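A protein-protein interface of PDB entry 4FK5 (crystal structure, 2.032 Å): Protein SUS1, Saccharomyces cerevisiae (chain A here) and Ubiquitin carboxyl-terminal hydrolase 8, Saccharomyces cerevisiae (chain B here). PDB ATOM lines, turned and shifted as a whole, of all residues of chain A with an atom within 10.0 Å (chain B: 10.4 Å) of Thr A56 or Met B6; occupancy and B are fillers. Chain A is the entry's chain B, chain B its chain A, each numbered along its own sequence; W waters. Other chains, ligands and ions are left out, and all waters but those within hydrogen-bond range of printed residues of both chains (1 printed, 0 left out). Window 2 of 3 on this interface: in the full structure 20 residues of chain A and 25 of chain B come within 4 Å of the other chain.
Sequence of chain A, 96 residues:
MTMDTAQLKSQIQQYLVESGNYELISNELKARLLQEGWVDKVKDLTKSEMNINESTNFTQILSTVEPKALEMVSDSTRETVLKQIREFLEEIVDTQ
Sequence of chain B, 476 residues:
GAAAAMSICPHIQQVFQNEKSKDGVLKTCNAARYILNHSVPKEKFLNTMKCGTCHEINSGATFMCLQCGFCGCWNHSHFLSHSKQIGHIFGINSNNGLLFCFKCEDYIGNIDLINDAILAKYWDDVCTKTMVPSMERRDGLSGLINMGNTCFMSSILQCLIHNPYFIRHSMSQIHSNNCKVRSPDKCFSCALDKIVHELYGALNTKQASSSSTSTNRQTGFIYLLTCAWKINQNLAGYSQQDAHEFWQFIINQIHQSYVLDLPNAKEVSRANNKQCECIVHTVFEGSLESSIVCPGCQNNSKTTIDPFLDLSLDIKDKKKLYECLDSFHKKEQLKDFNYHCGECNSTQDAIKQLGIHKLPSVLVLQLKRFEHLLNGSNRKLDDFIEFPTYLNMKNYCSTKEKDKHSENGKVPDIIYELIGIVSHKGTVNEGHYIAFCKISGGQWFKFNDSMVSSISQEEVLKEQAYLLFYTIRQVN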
ATOM      1  N   THR A  46       9.281  -3.254   1.123  1.00  0.00           N
ATOM      2  CA  THR A  46       8.925  -1.884   0.839  1.00  0.00           C
ATOM      3  C   THR A  46       7.406  -1.739   0.779  1.00  0.00           C
ATOM      4  O   THR A  46       6.860  -0.841   1.406  1.00  0.00           O
ATOM      5  CB  THR A  46       9.587  -1.370  -0.441  1.00  0.00           C
ATOM      6  OG1 THR A  46      11.025  -1.452  -0.285  1.00  0.00           O
ATOM      7  CG2 THR A  46       9.204   0.067  -0.685  1.00  0.00           C
ATOM      8  N   LYS A  47       6.741  -2.676   0.130  1.00  0.00           N
ATOM      9  CA  LYS A  47       5.321  -2.627   0.029  1.00  0.00           C
ATOM     10  C   LYS A  47       4.717  -2.755   1.428  1.00  0.00           C
ATOM     11  O   LYS A  47       3.795  -2.028   1.772  1.00  0.00           O
ATOM     12  CB  LYS A  47       4.798  -3.743  -0.864  1.00  0.00           C
ATOM     13  CG  LYS A  47       5.164  -3.555  -2.309  1.00  0.00           C
ATOM     14  CD  LYS A  47       4.536  -4.601  -3.202  1.00  0.00           C
ATOM     15  CE  LYS A  47       4.554  -4.170  -4.647  1.00  0.00           C
ATOM     16  NZ  LYS A  47       5.849  -4.579  -5.290  1.00  0.00           N
ATOM     17  N   SER A  48       5.298  -3.631   2.231  1.00  0.00           N
ATOM     18  CA  SER A  48       4.774  -3.911   3.496  1.00  0.00           C
ATOM     19  C   SER A  48       4.926  -2.682   4.352  1.00  0.00           C
ATOM     20  O   SER A  48       4.022  -2.334   5.096  1.00  0.00           O
ATOM     21  CB  SER A  48       5.474  -5.071   4.112  1.00  0.00           C
ATOM     22  OG  SER A  48       5.153  -5.135   5.473  1.00  0.00           O
ATOM     23  N   GLU A  49       6.046  -1.992   4.219  1.00  0.00           N
ATOM     24  CA  GLU A  49       6.262  -0.805   4.998  1.00  0.00           C
ATOM     25  C   GLU A  49       5.374   0.359   4.578  1.00  0.00           C
ATOM     26  O   GLU A  49       4.947   1.155   5.443  1.00  0.00           O
ATOM     27  CB  GLU A  49       7.731  -0.392   5.013  1.00  0.00           C
ATOM     28  CG  GLU A  49       8.637  -1.383   5.747  1.00  0.00           C
ATOM     29  CD  GLU A  49       8.448  -1.396   7.250  1.00  0.00           C
ATOM     30  OE1 GLU A  49       7.554  -0.694   7.782  1.00  0.00           O
ATOM     31  OE2 GLU A  49       9.205  -2.105   7.899  1.00  0.00           O
ATOM     32  N   MET A  50       5.052   0.462   3.292  1.00  0.00           N
ATOM     33  CA  MET A  50       4.053   1.459   2.845  1.00  0.00           C
ATOM     34  C   MET A  50       2.642   1.232   3.514  1.00  0.00           C
ATOM     35  O   MET A  50       1.948   2.204   3.907  1.00  0.00           O
ATOM     36  CB  MET A  50       3.910   1.451   1.325  1.00  0.00           C
ATOM     37  CG  MET A  50       5.165   1.943   0.616  1.00  0.00           C
ATOM     38  SD  MET A  50       4.957   2.311  -1.117  1.00  0.00           S
ATOM     39  CE  MET A  50       4.810   0.640  -1.825  1.00  0.00           C
ATOM     40  N   ASN A  51       2.210  -0.024   3.545  1.00  0.00           N
ATOM     41  CA  ASN A  51       0.967  -0.410   4.192  1.00  0.00           C
ATOM     42  C   ASN A  51       1.002  -0.073   5.687  1.00  0.00           C
ATOM     43  O   ASN A  51       0.130   0.579   6.206  1.00  0.00           O
ATOM     44  CB  ASN A  51       0.736  -1.914   4.038  1.00  0.00           C
ATOM     45  CG  ASN A  51      -0.506  -2.383   4.753  1.00  0.00           C
ATOM     46  OD1 ASN A  51      -1.616  -2.103   4.315  1.00  0.00           O
ATOM     47  ND2 ASN A  51      -0.328  -3.103   5.869  1.00  0.00           N
ATOM     48  N   ILE A  52       2.063  -0.502   6.350  1.00  0.00           N
ATOM     49  CA  ILE A  52       2.235  -0.255   7.748  1.00  0.00           C
ATOM     50  C   ILE A  52       2.109   1.221   8.134  1.00  0.00           C
ATOM     51  O   ILE A  52       1.391   1.550   9.101  1.00  0.00           O
ATOM     52  CB  ILE A  52       3.567  -0.835   8.255  1.00  0.00           C
ATOM     53  CG1 ILE A  52       3.441  -2.352   8.357  1.00  0.00           C
ATOM     54  CG2 ILE A  52       3.972  -0.238   9.608  1.00  0.00           C
ATOM     55  CD1 ILE A  52       4.725  -3.066   8.701  1.00  0.00           C
ATOM     56  N   ASN A  53       2.824   2.095   7.428  1.00  0.00           N
ATOM     57  CA  ASN A  53       2.924   3.522   7.814  1.00  0.00           C
ATOM     58  C   ASN A  53       1.918   4.365   7.062  1.00  0.00           C
ATOM     59  O   ASN A  53       1.928   5.627   7.164  1.00  0.00           O
ATOM     60  CB  ASN A  53       4.350   4.066   7.539  1.00  0.00           C
ATOM     61  CG  ASN A  53       5.417   3.413   8.411  1.00  0.00           C
ATOM     62  OD1 ASN A  53       5.557   3.739   9.594  1.00  0.00           O
ATOM     63  ND2 ASN A  53       6.179   2.460   7.822  1.00  0.00           N
ATOM     64  N   GLU A  54       1.106   3.693   6.239  1.00  0.00           N
ATOM     65  CA  GLU A  54       0.117   4.352   5.355  1.00  0.00           C
ATOM     66  C   GLU A  54       0.691   5.562   4.649  1.00  0.00           C
ATOM     67  O   GLU A  54       0.137   6.673   4.701  1.00  0.00           O
ATOM     68  CB  GLU A  54      -1.132   4.728   6.150  1.00  0.00           C
ATOM     69  CG  GLU A  54      -1.557   3.662   7.116  1.00  0.00           C
ATOM     70  CD  GLU A  54      -2.621   4.157   8.056  1.00  0.00           C
ATOM     71  OE1 GLU A  54      -3.812   3.903   7.767  1.00  0.00           O
ATOM     72  OE2 GLU A  54      -2.272   4.869   9.029  1.00  0.00           O
ATOM     73  N   SER A  55       1.779   5.329   3.912  1.00  0.00           N
ATOM     74  CA  SER A  55       2.477   6.376   3.299  1.00  0.00           C
ATOM     75  C   SER A  55       3.204   5.836   2.066  1.00  0.00           C
ATOM     76  O   SER A  55       3.610   4.660   2.031  1.00  0.00           O
ATOM     77  CB  SER A  55       3.462   6.994   4.298  1.00  0.00           C
ATOM     78  OG  SER A  55       4.092   8.144   3.739  1.00  0.00           O
ATOM     79  N   THR A  56       3.311   6.683   1.050  1.00  0.00           N
ATOM     80  CA  THR A  56       4.216   6.460  -0.073  1.00  0.00           C
ATOM     81  C   THR A  56       5.390   7.488  -0.066  1.00  0.00           C
ATOM     82  O   THR A  56       6.180   7.553  -1.029  1.00  0.00           O
ATOM     83  CB  THR A  56       3.445   6.547  -1.404  1.00  0.00           C
ATOM     84  OG1 THR A  56       2.826   7.826  -1.523  1.00  0.00           O
ATOM     85  CG2 THR A  56       2.372   5.437  -1.499  1.00  0.00           C
ATOM     86  N   ASN A  57       5.502   8.294   1.001  1.00  0.00           N
ATOM     87  CA  ASN A  57       6.565   9.318   1.062  1.00  0.00           C
ATOM     88  C   ASN A  57       7.934   8.663   1.095  1.00  0.00           C
ATOM     89  O   ASN A  57       8.260   7.915   2.055  1.00  0.00           O
ATOM     90  CB  ASN A  57       6.428  10.224   2.288  1.00  0.00           C
ATOM     91  CG  ASN A  57       7.501  11.290   2.333  1.00  0.00           C
ATOM     92  OD1 ASN A  57       7.300  12.385   1.826  1.00  0.00           O
ATOM     93  ND2 ASN A  57       8.676  10.958   2.905  1.00  0.00           N
ATOM     94  N   PHE A  58       8.746   8.933   0.064  1.00  0.00           N
ATOM     95  CA  PHE A  58      10.035   8.228  -0.107  1.00  0.00           C
ATOM     96  C   PHE A  58      10.945   8.346   1.109  1.00  0.00           C
ATOM     97  O   PHE A  58      11.467   7.344   1.596  1.00  0.00           O
ATOM     98  CB  PHE A  58      10.795   8.710  -1.381  1.00  0.00           C
ATOM     99  CG  PHE A  58      12.174   8.093  -1.523  1.00  0.00           C
ATOM    100  CD1 PHE A  58      12.318   6.796  -2.010  1.00  0.00           C
ATOM    101  CD2 PHE A  58      13.300   8.774  -1.074  1.00  0.00           C
ATOM    102  CE1 PHE A  58      13.564   6.200  -2.063  1.00  0.00           C
ATOM    103  CE2 PHE A  58      14.552   8.209  -1.156  1.00  0.00           C
ATOM    104  CZ  PHE A  58      14.693   6.921  -1.649  1.00  0.00           C
ATOM    105  N   THR A  59      11.106   9.552   1.639  1.00  0.00           N
ATOM    106  CA  THR A  59      12.030   9.781   2.749  1.00  0.00           C
ATOM    107  C   THR A  59      11.638   8.980   3.970  1.00  0.00           C
ATOM    108  O   THR A  59      12.478   8.368   4.638  1.00  0.00           O
ATOM    109  CB  THR A  59      12.085  11.279   3.096  1.00  0.00           C
ATOM    110  OG1 THR A  59      12.470  11.998   1.928  1.00  0.00           O
ATOM    111  CG2 THR A  59      13.108  11.590   4.268  1.00  0.00           C
ATOM    112  N   GLN A  60      10.356   8.970   4.260  1.00  0.00           N
ATOM    113  CA  GLN A  60       9.837   8.217   5.404  1.00  0.00           C
ATOM    114  C   GLN A  60       9.990   6.703   5.182  1.00  0.00           C
ATOM    115  O   GLN A  60      10.472   5.977   6.065  1.00  0.00           O
ATOM    116  CB  GLN A  60       8.338   8.577   5.641  1.00  0.00           C
ATOM    117  CG  GLN A  60       7.805   8.122   6.981  1.00  0.00           C
ATOM    118  CD  GLN A  60       6.269   8.232   7.093  1.00  0.00           C
ATOM    119  OE1 GLN A  60       5.653   7.499   7.874  1.00  0.00           O
ATOM    120  NE2 GLN A  60       5.646   9.145   6.289  1.00  0.00           N
ATOM    121  N   ILE A  61       9.594   6.227   3.998  1.00  0.00           N
ATOM    122  CA  ILE A  61       9.658   4.788   3.719  1.00  0.00           C
ATOM    123  C   ILE A  61      11.118   4.307   3.713  1.00  0.00           C
ATOM    124  O   ILE A  61      11.433   3.320   4.317  1.00  0.00           O
ATOM    125  CB  ILE A  61       8.947   4.414   2.418  1.00  0.00           C
ATOM    126  CG1 ILE A  61       7.487   4.814   2.467  1.00  0.00           C
ATOM    127  CG2 ILE A  61       9.033   2.917   2.162  1.00  0.00           C
ATOM    128  CD1 ILE A  61       6.743   4.181   3.635  1.00  0.00           C
ATOM    129  N   LEU A  62      12.019   5.051   3.076  1.00  0.00           N
ATOM    130  CA  LEU A  62      13.435   4.631   3.034  1.00  0.00           C
ATOM    131  C   LEU A  62      14.025   4.454   4.431  1.00  0.00           C
ATOM    132  O   LEU A  62      14.726   3.479   4.697  1.00  0.00           O
ATOM    133  CB  LEU A  62      14.275   5.647   2.211  1.00  0.00           C
ATOM    134  CG  LEU A  62      15.748   5.254   2.118  1.00  0.00           C
ATOM    135  CD1 LEU A  62      15.911   4.045   1.127  1.00  0.00           C
ATOM    136  CD2 LEU A  62      16.604   6.448   1.722  1.00  0.00           C
ATOM    137  N   ALA B   4      -8.816  11.880   2.711  1.00  0.00           N
ATOM    138  CA  ALA B   4      -8.156  10.607   2.332  1.00  0.00           C
ATOM    139  C   ALA B   4      -7.402  10.720   0.965  1.00  0.00           C
ATOM    140  O   ALA B   4      -6.527   9.908   0.674  1.00  0.00           O
ATOM    141  CB  ALA B   4      -9.189   9.479   2.297  1.00  0.00           C
ATOM    142  N   ALA B   5      -7.723  11.756   0.169  1.00  0.00           N
ATOM    143  CA  ALA B   5      -7.261  11.861  -1.243  1.00  0.00           C
ATOM    144  C   ALA B   5      -5.745  12.126  -1.351  1.00  0.00           C
ATOM    145  O   ALA B   5      -5.204  12.981  -0.652  1.00  0.00           O
ATOM    146  CB  ALA B   5      -8.045  12.956  -1.986  1.00  0.00           C
ATOM    147  N   MET B   6      -5.074  11.398  -2.251  1.00  0.00           N
ATOM    148  CA  MET B   6      -3.631  11.596  -2.487  1.00  0.00           C
ATOM    149  C   MET B   6      -3.404  12.851  -3.341  1.00  0.00           C
ATOM    150  O   MET B   6      -4.110  13.097  -4.334  1.00  0.00           O
ATOM    151  CB  MET B   6      -2.991  10.349  -3.165  1.00  0.00           C
ATOM    152  CG  MET B   6      -2.456   9.299  -2.182  1.00  0.00           C
ATOM    153  SD  MET B   6      -0.862   8.618  -2.702  1.00  0.00           S
ATOM    154  CE  MET B   6      -0.069   8.271  -1.128  1.00  0.00           C
ATOM    155  N   SER B   7      -2.413  13.636  -2.957  1.00  0.00           N
ATOM    156  CA  SER B   7      -2.210  14.940  -3.542  1.00  0.00           C
ATOM    157  C   SER B   7      -0.994  14.976  -4.450  1.00  0.00           C
ATOM    158  O   SER B   7      -0.224  14.035  -4.510  1.00  0.00           O
ATOM    159  CB  SER B   7      -2.036  15.945  -2.437  1.00  0.00           C
ATOM    160  OG  SER B   7      -1.127  15.439  -1.497  1.00  0.00           O
ATOM    161  N   ILE B   8      -0.842  16.076  -5.155  1.00  0.00           N
ATOM    162  CA  ILE B   8       0.247  16.250  -6.098  1.00  0.00           C
ATOM    163  C   ILE B   8       1.233  17.237  -5.510  1.00  0.00           C
ATOM    164  O   ILE B   8       0.852  18.090  -4.710  1.00  0.00           O
ATOM    165  CB  ILE B   8      -0.291  16.766  -7.447  1.00  0.00           C
ATOM    166  CG1 ILE B   8      -1.229  15.710  -8.076  1.00  0.00           C
ATOM    167  CG2 ILE B   8       0.850  17.080  -8.387  1.00  0.00           C
ATOM    168  CD1 ILE B   8      -2.520  16.288  -8.648  1.00  0.00           C
ATOM    169  N   CYS B   9       2.507  17.101  -5.869  1.00  0.00           N
ATOM    170  CA  CYS B   9       3.510  18.035  -5.435  1.00  0.00           C
ATOM    171  C   CYS B   9       3.025  19.429  -5.818  1.00  0.00           C
ATOM    172  O   CYS B   9       2.810  19.704  -7.006  1.00  0.00           O
ATOM    173  CB  CYS B   9       4.879  17.768  -6.096  1.00  0.00           C
ATOM    174  SG  CYS B   9       6.031  19.168  -5.973  1.00  0.00           S
ATOM    175  N   PRO B  10       2.866  20.323  -4.822  1.00  0.00           N
ATOM    176  CA  PRO B  10       2.358  21.662  -5.154  1.00  0.00           C
ATOM    177  C   PRO B  10       3.367  22.521  -5.938  1.00  0.00           C
ATOM    178  O   PRO B  10       2.960  23.417  -6.735  1.00  0.00           O
ATOM    179  CB  PRO B  10       2.038  22.274  -3.767  1.00  0.00           C
ATOM    180  CG  PRO B  10       2.925  21.544  -2.817  1.00  0.00           C
ATOM    181  CD  PRO B  10       3.077  20.149  -3.375  1.00  0.00           C
ATOM    182  N   GLN B  13       3.386  21.743  -9.669  1.00  0.00           N
ATOM    183  CA  GLN B  13       2.067  22.290 -10.146  1.00  0.00           C
ATOM    184  C   GLN B  13       2.139  23.810 -10.398  1.00  0.00           C
ATOM    185  O   GLN B  13       1.665  24.315 -11.431  1.00  0.00           O
ATOM    186  CB  GLN B  13       0.978  22.026  -9.128  1.00  0.00           C
ATOM    187  CG  GLN B  13       0.264  20.707  -9.292  1.00  0.00           C
ATOM    188  CD  GLN B  13      -0.804  20.531  -8.254  1.00  0.00           C
ATOM    189  OE1 GLN B  13      -0.697  19.674  -7.377  1.00  0.00           O
ATOM    190  NE2 GLN B  13      -1.810  21.393  -8.293  1.00  0.00           N
ATOM    191  N   LEU B  98      13.697   8.974 -12.267  1.00  0.00           N
ATOM    192  CA  LEU B  98      12.542   9.518 -11.534  1.00  0.00           C
ATOM    193  C   LEU B  98      12.873  10.897 -10.939  1.00  0.00           C
ATOM    194  O   LEU B  98      14.029  11.194 -10.612  1.00  0.00           O
ATOM    195  CB  LEU B  98      12.059   8.574 -10.438  1.00  0.00           C
ATOM    196  CG  LEU B  98      11.601   7.176 -10.830  1.00  0.00           C
ATOM    197  CD1 LEU B  98      11.557   6.303  -9.574  1.00  0.00           C
ATOM    198  CD2 LEU B  98      10.273   7.165 -11.600  1.00  0.00           C
ATOM    199  N   LEU B  99      11.845  11.737 -10.871  1.00  0.00           N
ATOM    200  CA  LEU B  99      11.988  13.156 -10.542  1.00  0.00           C
ATOM    201  C   LEU B  99      11.648  13.366  -9.060  1.00  0.00           C
ATOM    202  O   LEU B  99      10.573  13.026  -8.630  1.00  0.00           O
ATOM    203  CB  LEU B  99      11.064  14.005 -11.446  1.00  0.00           C
ATOM    204  CG  LEU B  99      11.152  15.557 -11.306  1.00  0.00           C
ATOM    205  CD1 LEU B  99      12.539  16.087 -11.722  1.00  0.00           C
ATOM    206  CD2 LEU B  99      10.016  16.221 -12.114  1.00  0.00           C
ATOM    207  N   PHE B 100      12.602  13.910  -8.307  1.00  0.00           N
ATOM    208  CA  PHE B 100      12.455  14.127  -6.852  1.00  0.00           C
ATOM    209  C   PHE B 100      12.235  15.623  -6.578  1.00  0.00           C
ATOM    210  O   PHE B 100      12.897  16.446  -7.143  1.00  0.00           O
ATOM    211  CB  PHE B 100      13.719  13.687  -6.110  1.00  0.00           C
ATOM    212  CG  PHE B 100      13.533  13.470  -4.624  1.00  0.00           C
ATOM    213  CD1 PHE B 100      12.994  12.298  -4.143  1.00  0.00           C
ATOM    214  CD2 PHE B 100      14.008  14.398  -3.706  1.00  0.00           C
ATOM    215  CE1 PHE B 100      12.900  12.070  -2.781  1.00  0.00           C
ATOM    216  CE2 PHE B 100      13.912  14.163  -2.347  1.00  0.00           C
ATOM    217  CZ  PHE B 100      13.355  13.009  -1.895  1.00  0.00           C
ATOM    218  N   CYS B 104       9.201  18.705  -0.984  1.00  0.00           N
ATOM    219  CA  CYS B 104       8.320  17.633  -0.503  1.00  0.00           C
ATOM    220  C   CYS B 104       9.083  16.472   0.110  1.00  0.00           C
ATOM    221  O   CYS B 104       8.501  15.667   0.784  1.00  0.00           O
ATOM    222  CB  CYS B 104       7.445  17.053  -1.632  1.00  0.00           C
ATOM    223  SG  CYS B 104       6.333  18.212  -2.449  1.00  0.00           S
ATOM    224  N   GLU B 105      10.380  16.348  -0.200  1.00  0.00           N
ATOM    225  CA  GLU B 105      11.157  15.182   0.229  1.00  0.00           C
ATOM    226  C   GLU B 105      10.503  13.883  -0.239  1.00  0.00           C
ATOM    227  O   GLU B 105      10.503  12.910   0.444  1.00  0.00           O
ATOM    228  CB  GLU B 105      11.361  15.204   1.739  1.00  0.00           C
ATOM    229  CG  GLU B 105      12.043  16.494   2.166  1.00  0.00           C
ATOM    230  CD  GLU B 105      12.771  16.396   3.478  1.00  0.00           C
ATOM    231  OE1 GLU B 105      13.770  17.146   3.641  1.00  0.00           O
ATOM    232  OE2 GLU B 105      12.312  15.635   4.371  1.00  0.00           O
ATOM    233  N   ASP B 106       9.997  13.924  -1.456  1.00  0.00           N
ATOM    234  CA  ASP B 106       9.373  12.801  -2.095  1.00  0.00           C
ATOM    235  C   ASP B 106       9.569  12.865  -3.643  1.00  0.00           C
ATOM    236  O   ASP B 106       9.801  13.967  -4.229  1.00  0.00           O
ATOM    237  CB  ASP B 106       7.904  12.853  -1.803  1.00  0.00           C
ATOM    238  CG  ASP B 106       7.222  11.563  -2.004  1.00  0.00           C
ATOM    239  OD1 ASP B 106       7.912  10.472  -2.126  1.00  0.00           O
ATOM    240  OD2 ASP B 106       5.960  11.599  -1.964  1.00  0.00           O
ATOM    241  N   TYR B 107       9.429  11.712  -4.293  1.00  0.00           N
ATOM    242  CA  TYR B 107       9.360  11.665  -5.719  1.00  0.00           C
ATOM    243  C   TYR B 107       8.034  12.162  -6.204  1.00  0.00           C
ATOM    244  O   TYR B 107       7.016  11.962  -5.575  1.00  0.00           O
ATOM    245  CB  TYR B 107       9.619  10.234  -6.277  1.00  0.00           C
ATOM    246  CG  TYR B 107      11.035   9.834  -6.229  1.00  0.00           C
ATOM    247  CD1 TYR B 107      11.917  10.247  -7.219  1.00  0.00           C
ATOM    248  CD2 TYR B 107      11.557   9.178  -5.129  1.00  0.00           C
ATOM    249  CE1 TYR B 107      13.269   9.964  -7.149  1.00  0.00           C
ATOM    250  CE2 TYR B 107      12.931   8.895  -5.039  1.00  0.00           C
ATOM    251  CZ  TYR B 107      13.772   9.261  -6.075  1.00  0.00           C
ATOM    252  OH  TYR B 107      15.120   8.978  -6.021  1.00  0.00           O
ATOM    253  N   ILE B 108       8.056  12.749  -7.386  1.00  0.00           N
ATOM    254  CA  ILE B 108       6.838  13.063  -8.100  1.00  0.00           C
ATOM    255  C   ILE B 108       6.462  11.907  -9.043  1.00  0.00           C
ATOM    256  O   ILE B 108       7.002  11.783 -10.133  1.00  0.00           O
ATOM    257  CB  ILE B 108       7.028  14.337  -8.906  1.00  0.00           C
ATOM    258  CG1 ILE B 108       7.408  15.515  -7.958  1.00  0.00           C
ATOM    259  CG2 ILE B 108       5.769  14.637  -9.718  1.00  0.00           C
ATOM    260  CD1 ILE B 108       8.044  16.738  -8.679  1.00  0.00           C
ATOM    261  N   GLY B 109       5.587  11.015  -8.588  1.00  0.00           N
ATOM    262  CA  GLY B 109       5.349   9.764  -9.326  1.00  0.00           C
ATOM    263  C   GLY B 109       3.954   9.674  -9.926  1.00  0.00           C
ATOM    264  O   GLY B 109       3.643   8.723 -10.650  1.00  0.00           O
ATOM    265  N   ASN B 110       3.088  10.641  -9.598  1.00  0.00           N
ATOM    266  CA  ASN B 110       1.703  10.534  -9.970  1.00  0.00           C
ATOM    267  C   ASN B 110       1.203  11.555 -10.989  1.00  0.00           C
ATOM    268  O   ASN B 110       0.046  11.769 -11.090  1.00  0.00           O
ATOM    269  CB  ASN B 110       0.837  10.557  -8.745  1.00  0.00           C
ATOM    270  CG  ASN B 110       0.990  11.841  -7.914  1.00  0.00           C
ATOM    271  OD1 ASN B 110       1.742  12.774  -8.264  1.00  0.00           O
ATOM    272  ND2 ASN B 110       0.278  11.879  -6.806  1.00  0.00           N
ATOM    273  N   ILE B 111       2.089  12.147 -11.753  1.00  0.00           N
ATOM    274  CA  ILE B 111       1.683  13.027 -12.855  1.00  0.00           C
ATOM    275  C   ILE B 111       1.956  12.323 -14.192  1.00  0.00           C
ATOM    276  O   ILE B 111       3.151  12.063 -14.554  1.00  0.00           O
ATOM    277  CB  ILE B 111       2.472  14.348 -12.785  1.00  0.00           C
ATOM    278  CG1 ILE B 111       2.164  15.057 -11.474  1.00  0.00           C
ATOM    279  CG2 ILE B 111       2.201  15.227 -14.023  1.00  0.00           C
ATOM    280  CD1 ILE B 111       2.990  16.320 -11.247  1.00  0.00           C
HETATM  281  O   HOH W   1       8.191   8.350  -3.724  1.00  0.00           O
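The side-chain hydroxyl (OG) of Ser A55 is in hydrogen-bond range of the backbone NH (N) of Asn A57 (3.1 Å). The side-chain amide nitrogen (ND2) of Asn A57 sits close to the backbone NH (N) of Thr A59. The side-chain amide nitrogen (ND2) of Asn A57 sits close to the backbone NH (N) of Gln A60 (2.9 Å).
Of the 19 printed residues of chain B, 6 touch a printed residue of chain A. Hydrophobic or aromatic side chains of chain B that line the printed part of chain A: Met B6, Phe B100 and Tyr B107. Hydrophobic or aromatic side chains of chain A within 4 Å of the printed part of chain B: Phe A58.
Thr A56 touches just these residues of chain B: Met B6 (3.0 Å) and Asp B106 (3.6 Å). Of chain A, only Thr A56 comes within 4 Å of Met B6. No residue of chain A comes within 4 Å of Ala B5. Printed residues of chain A within 4 Å of Asp B106: Thr A56, Asn A57 and Phe A58. Of the printed residues of chain A, Glu B105 touches Asn A57 (3.5 Å) and Thr A59 (2.6 Å). Printed residues of chain A within 4 Å of Phe B100: Phe A58. Printed residues of chain B within 4 Å of Thr A59: Glu B105 (2.6 Å). Of the printed residues of chain A, Cys B104 touches Asn A57 (3.6 Å). Glu A54 touches none of the printed residues of chain B. Thr A46 touches none of the printed residues of chain B. The nearest residue of chain A that does not touch Met B6 is Ser A55 (5.2 Å). The nearest printed residue of chain B that does not touch Thr A59 is Phe B100 (4.1 Å).
Thr A56 touches Met B6. Thr A56 touches Asp B106 (O to OD1, 3.6 Å). OD1 of Asn A57 touches O of Cys B104 (3.6 Å). Asn A57 touches Glu B105 (OD1 to O, 3.5 Å). CA of Asn A57 touches OD1 of Asp B106, 3.6 Å away. Phe A58 touches Phe B100 (CD2 to CE1, 3.7 Å). CG of Phe A58 touches CE2 of Tyr B107 (3.7 Å).
Water W1 lies within hydrogen-bond range of OD1 of Asp B106 (2.7 Å) and O of Thr A56 (3.5 Å).
OG1 of Thr A59 lies within hydrogen-bond range of O of Glu B105. The backbone NH (N) of Phe A58 is in hydrogen-bond range of the side-chain carboxylate (OD1) of Asp B106, 2.8 Å away.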
